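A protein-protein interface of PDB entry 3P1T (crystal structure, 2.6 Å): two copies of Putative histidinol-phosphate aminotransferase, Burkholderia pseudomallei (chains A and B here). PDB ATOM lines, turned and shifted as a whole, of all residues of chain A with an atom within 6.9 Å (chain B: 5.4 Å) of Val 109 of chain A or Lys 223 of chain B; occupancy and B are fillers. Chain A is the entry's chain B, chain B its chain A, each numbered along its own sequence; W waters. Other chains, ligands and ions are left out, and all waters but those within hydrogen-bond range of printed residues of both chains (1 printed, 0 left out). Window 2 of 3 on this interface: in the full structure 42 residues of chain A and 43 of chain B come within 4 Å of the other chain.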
ATOM      1  N   ASP A  78     -30.616  -4.120  15.325  1.00  0.00           N
ATOM      2  CA  ASP A  78     -29.559  -3.501  14.503  1.00  0.00           C
ATOM      3  C   ASP A  78     -29.463  -4.193  13.143  1.00  0.00           C
ATOM      4  O   ASP A  78     -29.515  -3.487  12.128  1.00  0.00           O
ATOM      5  CB  ASP A  78     -28.178  -3.495  15.183  1.00  0.00           C
ATOM      6  CG  ASP A  78     -27.967  -2.535  16.336  1.00  0.00           C
ATOM      7  OD1 ASP A  78     -28.972  -2.061  16.909  1.00  0.00           O
ATOM      8  OD2 ASP A  78     -26.799  -2.317  16.716  1.00  0.00           O
ATOM      9  N   ASP A  82     -30.647  -2.526   9.429  1.00  0.00           N
ATOM     10  CA  ASP A  82     -29.649  -2.463   8.364  1.00  0.00           C
ATOM     11  C   ASP A  82     -30.099  -3.181   7.105  1.00  0.00           C
ATOM     12  O   ASP A  82     -30.018  -2.598   6.032  1.00  0.00           O
ATOM     13  CB  ASP A  82     -28.306  -3.063   8.821  1.00  0.00           C
ATOM     14  CG  ASP A  82     -27.457  -2.165   9.678  1.00  0.00           C
ATOM     15  OD1 ASP A  82     -27.945  -1.068  10.052  1.00  0.00           O
ATOM     16  OD2 ASP A  82     -26.277  -2.536   9.938  1.00  0.00           O
ATOM     17  N   ARG A 104     -31.622   5.974  15.168  1.00  0.00           N
ATOM     18  CA  ARG A 104     -30.738   7.117  14.908  1.00  0.00           C
ATOM     19  C   ARG A 104     -29.296   6.688  14.613  1.00  0.00           C
ATOM     20  O   ARG A 104     -28.660   7.245  13.714  1.00  0.00           O
ATOM     21  CB  ARG A 104     -30.715   8.062  16.116  1.00  0.00           C
ATOM     22  CG  ARG A 104     -31.640   9.230  16.020  1.00  0.00           C
ATOM     23  CD  ARG A 104     -31.408  10.146  17.192  1.00  0.00           C
ATOM     24  NE  ARG A 104     -32.143  11.396  17.012  1.00  0.00           N
ATOM     25  CZ  ARG A 104     -31.882  12.534  17.649  1.00  0.00           C
ATOM     26  NH1 ARG A 104     -30.873  12.608  18.502  1.00  0.00           N
ATOM     27  NH2 ARG A 104     -32.613  13.610  17.418  1.00  0.00           N
ATOM     28  N   ALA A 105     -28.785   5.720  15.401  1.00  0.00           N
ATOM     29  CA  ALA A 105     -27.423   5.213  15.330  1.00  0.00           C
ATOM     30  C   ALA A 105     -27.167   4.511  14.006  1.00  0.00           C
ATOM     31  O   ALA A 105     -26.121   4.723  13.399  1.00  0.00           O
ATOM     32  CB  ALA A 105     -27.173   4.260  16.488  1.00  0.00           C
ATOM     33  N   ARG A 106     -28.130   3.703  13.548  1.00  0.00           N
ATOM     34  CA  ARG A 106     -28.024   2.956  12.292  1.00  0.00           C
ATOM     35  C   ARG A 106     -28.159   3.890  11.078  1.00  0.00           C
ATOM     36  O   ARG A 106     -27.525   3.635  10.057  1.00  0.00           O
ATOM     37  CB  ARG A 106     -29.085   1.838  12.243  1.00  0.00           C
ATOM     38  CG  ARG A 106     -28.876   0.724  13.283  1.00  0.00           C
ATOM     39  CD  ARG A 106     -27.753  -0.204  12.873  1.00  0.00           C
ATOM     40  NE  ARG A 106     -26.497   0.092  13.545  1.00  0.00           N
ATOM     41  CZ  ARG A 106     -25.299  -0.296  13.120  1.00  0.00           C
ATOM     42  NH1 ARG A 106     -25.165  -0.914  11.954  1.00  0.00           N
ATOM     43  NH2 ARG A 106     -24.220  -0.008  13.826  1.00  0.00           N
ATOM     44  N   ILE A 107     -28.963   4.967  11.190  1.00  0.00           N
ATOM     45  CA  ILE A 107     -29.151   5.976  10.135  1.00  0.00           C
ATOM     46  C   ILE A 107     -27.828   6.752   9.983  1.00  0.00           C
ATOM     47  O   ILE A 107     -27.436   7.106   8.867  1.00  0.00           O
ATOM     48  CB  ILE A 107     -30.374   6.889  10.467  1.00  0.00           C
ATOM     49  CG1 ILE A 107     -31.672   6.152  10.104  1.00  0.00           C
ATOM     50  CG2 ILE A 107     -30.319   8.220   9.713  1.00  0.00           C
ATOM     51  CD1 ILE A 107     -32.940   6.581  10.804  1.00  0.00           C
ATOM     52  N   ALA A 108     -27.114   6.936  11.101  1.00  0.00           N
ATOM     53  CA  ALA A 108     -25.834   7.634  11.151  1.00  0.00           C
ATOM     54  C   ALA A 108     -24.762   6.879  10.358  1.00  0.00           C
ATOM     55  O   ALA A 108     -24.069   7.496   9.544  1.00  0.00           O
ATOM     56  CB  ALA A 108     -25.393   7.811  12.605  1.00  0.00           C
ATOM     57  N   VAL A 109     -24.727   5.537  10.481  1.00  0.00           N
ATOM     58  CA  VAL A 109     -23.708   4.733   9.829  1.00  0.00           C
ATOM     59  C   VAL A 109     -24.048   4.527   8.333  1.00  0.00           C
ATOM     60  O   VAL A 109     -23.138   4.201   7.591  1.00  0.00           O
ATOM     61  CB  VAL A 109     -23.433   3.366  10.547  1.00  0.00           C
ATOM     62  CG1 VAL A 109     -23.002   3.566  11.999  1.00  0.00           C
ATOM     63  CG2 VAL A 109     -24.608   2.412  10.486  1.00  0.00           C
ATOM     64  N   SER A 110     -25.295   4.789   7.874  1.00  0.00           N
ATOM     65  CA  SER A 110     -25.703   4.574   6.474  1.00  0.00           C
ATOM     66  C   SER A 110     -25.870   5.858   5.630  1.00  0.00           C
ATOM     67  O   SER A 110     -25.877   5.774   4.398  1.00  0.00           O
ATOM     68  CB  SER A 110     -27.024   3.834   6.434  1.00  0.00           C
ATOM     69  OG  SER A 110     -26.876   2.509   6.912  1.00  0.00           O
ATOM     70  N   GLY A 111     -26.035   7.005   6.281  1.00  0.00           N
ATOM     71  CA  GLY A 111     -26.189   8.303   5.629  1.00  0.00           C
ATOM     72  C   GLY A 111     -27.485   8.425   4.869  1.00  0.00           C
ATOM     73  O   GLY A 111     -27.504   8.960   3.760  1.00  0.00           O
ATOM     74  N   LEU A 112     -28.574   7.945   5.473  1.00  0.00           N
ATOM     75  CA  LEU A 112     -29.907   7.932   4.875  1.00  0.00           C
ATOM     76  C   LEU A 112     -30.672   9.211   5.181  1.00  0.00           C
ATOM     77  O   LEU A 112     -30.402   9.847   6.195  1.00  0.00           O
ATOM     78  CB  LEU A 112     -30.674   6.725   5.437  1.00  0.00           C
ATOM     79  CG  LEU A 112     -30.116   5.313   5.150  1.00  0.00           C
ATOM     80  CD1 LEU A 112     -30.743   4.317   6.054  1.00  0.00           C
ATOM     81  CD2 LEU A 112     -30.323   4.892   3.720  1.00  0.00           C
ATOM     82  N   ARG B  83     -17.276  -5.567   6.405  1.00  0.00           N
ATOM     83  CA  ARG B  83     -16.944  -4.326   7.098  1.00  0.00           C
ATOM     84  C   ARG B  83     -15.703  -3.663   6.462  1.00  0.00           C
ATOM     85  O   ARG B  83     -15.681  -2.440   6.371  1.00  0.00           O
ATOM     86  CB  ARG B  83     -16.758  -4.559   8.600  1.00  0.00           C
ATOM     87  CG  ARG B  83     -18.037  -5.119   9.212  1.00  0.00           C
ATOM     88  CD  ARG B  83     -18.513  -4.394  10.445  1.00  0.00           C
ATOM     89  NE  ARG B  83     -19.762  -4.967  10.948  1.00  0.00           N
ATOM     90  CZ  ARG B  83     -20.972  -4.556  10.580  1.00  0.00           C
ATOM     91  NH1 ARG B  83     -21.110  -3.566   9.708  1.00  0.00           N
ATOM     92  NH2 ARG B  83     -22.051  -5.121  11.087  1.00  0.00           N
ATOM     93  N   ALA B  86     -16.890  -2.179   2.960  1.00  0.00           N
ATOM     94  CA  ALA B  86     -17.730  -0.989   3.180  1.00  0.00           C
ATOM     95  C   ALA B  86     -16.870   0.297   3.374  1.00  0.00           C
ATOM     96  O   ALA B  86     -17.356   1.400   3.115  1.00  0.00           O
ATOM     97  CB  ALA B  86     -18.635  -1.194   4.385  1.00  0.00           C
ATOM     98  N   GLU B  87     -15.601   0.149   3.784  1.00  0.00           N
ATOM     99  CA  GLU B  87     -14.693   1.279   3.997  1.00  0.00           C
ATOM    100  C   GLU B  87     -13.879   1.598   2.743  1.00  0.00           C
ATOM    101  O   GLU B  87     -13.311   2.687   2.672  1.00  0.00           O
ATOM    102  CB  GLU B  87     -13.728   0.994   5.181  1.00  0.00           C
ATOM    103  CG  GLU B  87     -14.413   0.764   6.525  1.00  0.00           C
ATOM    104  CD  GLU B  87     -15.380   1.839   6.984  1.00  0.00           C
ATOM    105  OE1 GLU B  87     -15.016   3.041   6.967  1.00  0.00           O
ATOM    106  OE2 GLU B  87     -16.520   1.475   7.353  1.00  0.00           O
ATOM    107  N   ALA B 219     -13.347   2.861  13.293  1.00  0.00           N
ATOM    108  CA  ALA B 219     -14.453   3.235  12.404  1.00  0.00           C
ATOM    109  C   ALA B 219     -15.345   2.022  12.069  1.00  0.00           C
ATOM    110  O   ALA B 219     -16.565   2.190  11.943  1.00  0.00           O
ATOM    111  CB  ALA B 219     -13.916   3.853  11.127  1.00  0.00           C
ATOM    112  N   MET B 220     -14.748   0.812  11.922  1.00  0.00           N
ATOM    113  CA  MET B 220     -15.523  -0.390  11.624  1.00  0.00           C
ATOM    114  C   MET B 220     -16.264  -0.863  12.892  1.00  0.00           C
ATOM    115  O   MET B 220     -17.425  -1.264  12.779  1.00  0.00           O
ATOM    116  CB  MET B 220     -14.641  -1.517  11.045  1.00  0.00           C
ATOM    117  CG  MET B 220     -14.158  -1.267   9.627  1.00  0.00           C
ATOM    118  SD  MET B 220     -13.069  -2.734   8.966  1.00  0.00           S
ATOM    119  CE  MET B 220     -11.630  -2.639  10.174  1.00  0.00           C
ATOM    120  N   LYS B 221     -15.611  -0.800  14.090  1.00  0.00           N
ATOM    121  CA  LYS B 221     -16.218  -1.153  15.390  1.00  0.00           C
ATOM    122  C   LYS B 221     -17.486  -0.364  15.611  1.00  0.00           C
ATOM    123  O   LYS B 221     -18.480  -0.920  16.070  1.00  0.00           O
ATOM    124  CB  LYS B 221     -15.248  -0.921  16.560  1.00  0.00           C
ATOM    125  CG  LYS B 221     -14.214  -2.023  16.716  1.00  0.00           C
ATOM    126  CD  LYS B 221     -13.325  -1.782  17.900  1.00  0.00           C
ATOM    127  CE  LYS B 221     -12.342  -2.909  18.056  1.00  0.00           C
ATOM    128  NZ  LYS B 221     -11.424  -2.716  19.210  1.00  0.00           N
ATOM    129  N   ARG B 222     -17.460   0.918  15.220  1.00  0.00           N
ATOM    130  CA  ARG B 222     -18.584   1.862  15.270  1.00  0.00           C
ATOM    131  C   ARG B 222     -19.789   1.367  14.431  1.00  0.00           C
ATOM    132  O   ARG B 222     -20.938   1.660  14.763  1.00  0.00           O
ATOM    133  CB  ARG B 222     -18.130   3.251  14.756  1.00  0.00           C
ATOM    134  CG  ARG B 222     -18.011   4.315  15.832  1.00  0.00           C
ATOM    135  CD  ARG B 222     -17.527   5.656  15.293  1.00  0.00           C
ATOM    136  NE  ARG B 222     -16.064   5.753  15.257  1.00  0.00           N
ATOM    137  CZ  ARG B 222     -15.348   6.144  14.200  1.00  0.00           C
ATOM    138  NH1 ARG B 222     -15.955   6.470  13.058  1.00  0.00           N
ATOM    139  NH2 ARG B 222     -14.025   6.199  14.271  1.00  0.00           N
ATOM    140  N   LYS B 223     -19.521   0.605  13.364  1.00  0.00           N
ATOM    141  CA  LYS B 223     -20.587   0.124  12.479  1.00  0.00           C
ATOM    142  C   LYS B 223     -21.097  -1.267  12.906  1.00  0.00           C
ATOM    143  O   LYS B 223     -22.167  -1.676  12.444  1.00  0.00           O
ATOM    144  CB  LYS B 223     -20.118   0.105  11.004  1.00  0.00           C
ATOM    145  CG  LYS B 223     -19.960   1.524  10.464  1.00  0.00           C
ATOM    146  CD  LYS B 223     -19.482   1.605   9.060  1.00  0.00           C
ATOM    147  CE  LYS B 223     -19.360   3.044   8.642  1.00  0.00           C
ATOM    148  NZ  LYS B 223     -19.067   3.165   7.195  1.00  0.00           N
ATOM    149  N   GLN B 224     -20.399  -1.943  13.830  1.00  0.00           N
ATOM    150  CA  GLN B 224     -20.810  -3.269  14.296  1.00  0.00           C
ATOM    151  C   GLN B 224     -22.109  -3.194  15.085  1.00  0.00           C
ATOM    152  O   GLN B 224     -22.480  -2.137  15.608  1.00  0.00           O
ATOM    153  CB  GLN B 224     -19.730  -3.939  15.135  1.00  0.00           C
ATOM    154  CG  GLN B 224     -18.508  -4.367  14.338  1.00  0.00           C
ATOM    155  CD  GLN B 224     -17.591  -5.213  15.181  1.00  0.00           C
ATOM    156  OE1 GLN B 224     -16.907  -4.724  16.099  1.00  0.00           O
ATOM    157  NE2 GLN B 224     -17.608  -6.517  14.923  1.00  0.00           N
ATOM    158  N   TRP B 225     -22.822  -4.315  15.123  1.00  0.00           N
ATOM    159  CA  TRP B 225     -24.099  -4.388  15.793  1.00  0.00           C
ATOM    160  C   TRP B 225     -23.912  -4.468  17.277  1.00  0.00           C
ATOM    161  O   TRP B 225     -22.890  -4.974  17.744  1.00  0.00           O
ATOM    162  CB  TRP B 225     -24.884  -5.596  15.291  1.00  0.00           C
ATOM    163  CG  TRP B 225     -25.149  -5.601  13.812  1.00  0.00           C
ATOM    164  CD1 TRP B 225     -25.451  -4.524  13.031  1.00  0.00           C
ATOM    165  CD2 TRP B 225     -25.298  -6.761  12.972  1.00  0.00           C
ATOM    166  NE1 TRP B 225     -25.688  -4.929  11.740  1.00  0.00           N
ATOM    167  CE2 TRP B 225     -25.621  -6.300  11.679  1.00  0.00           C
ATOM    168  CE3 TRP B 225     -25.125  -8.152  13.175  1.00  0.00           C
ATOM    169  CZ2 TRP B 225     -25.793  -7.171  10.598  1.00  0.00           C
ATOM    170  CZ3 TRP B 225     -25.321  -9.020  12.110  1.00  0.00           C
ATOM    171  CH2 TRP B 225     -25.635  -8.530  10.838  1.00  0.00           C
HETATM  172  O   HOH W   1     -23.851  -3.393   9.023  1.00  0.00           O
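Of the 10 printed residues of chain B, 4 touch a printed residue of chain A. Hydrophobic or aromatic side chains of chain B that line the printed part of chain A: Trp 225. Hydrophobic or aromatic side chains of chain A within 4 Å of the printed part of chain B: Val 109. Among the printed residues, 8 pairs touch across the chains.
Among the printed residues, merely in contact across the chains: Asp 78 of chain A with Trp 225 of chain B (3.5 Å), Arg 106 of chain A with Arg 222 of chain B (3.8 Å), Arg 106 of chain A with Trp 225 of chain B (3.8 Å), Val 109 of chain A with Arg 222 of chain B (3.9 Å) and Val 109 of chain A with Lys 223 of chain B (3.9 Å).
Water W1 lies within hydrogen-bond range of OD2 of Asp 82 of chain A and NH1 of Arg 83 of chain B.
No position is printed for both chains.
Val 109 of chain A touches two residues of chain B. Lys 223 of chain B touches two residues of chain A. Printed residues of chain A within 4 Å of Gln 224 of chain B: Arg 106 (3.3 Å). Printed residues of chain B within 4 Å of Asp 82 of chain A: Trp 225 (3.1 Å). The nearest printed residue of chain A that does not touch Trp 225 of chain B is Val 109 of chain A (7.4 Å).
The backbone carbonyl oxygen (O) of Lys 223 of chain B is in hydrogen-bond range of the guanidinium group (NH2) of Arg 106 of chain A (3.0 Å). NH2 of Arg 106 of chain A lies within hydrogen-bond range of O of Gln 224 of chain B. The indole nitrogen of Trp 225 of chain B is in hydrogen-bond range of the side-chain carboxylate of Asp 82 of chain A (3.1 Å).
The guanidinium group (NE) of Arg 106 of chain A lies within salt-bridge range of the side-chain carboxylate (OD2) of Asp 78 of chain A, at 3.99 Å. The guanidinium group of Arg 83 of chain B sits at hydrogen-bond distance from the backbone carbonyl oxygen of Lys 223 of chain B (3.5 Å). The side-chain amino group of Lys 223 of chain B is in salt-bridge range of the side-chain carboxylate of Glu 87 of chain B. OG of Ser 110 of chain A lies within hydrogen-bond range of O of Arg 106 of chain A, 3.4 Å away. NH1 of Arg 106 of chain A lies within salt-bridge range of OD2 of Asp 82 of chain A (2.8 Å).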
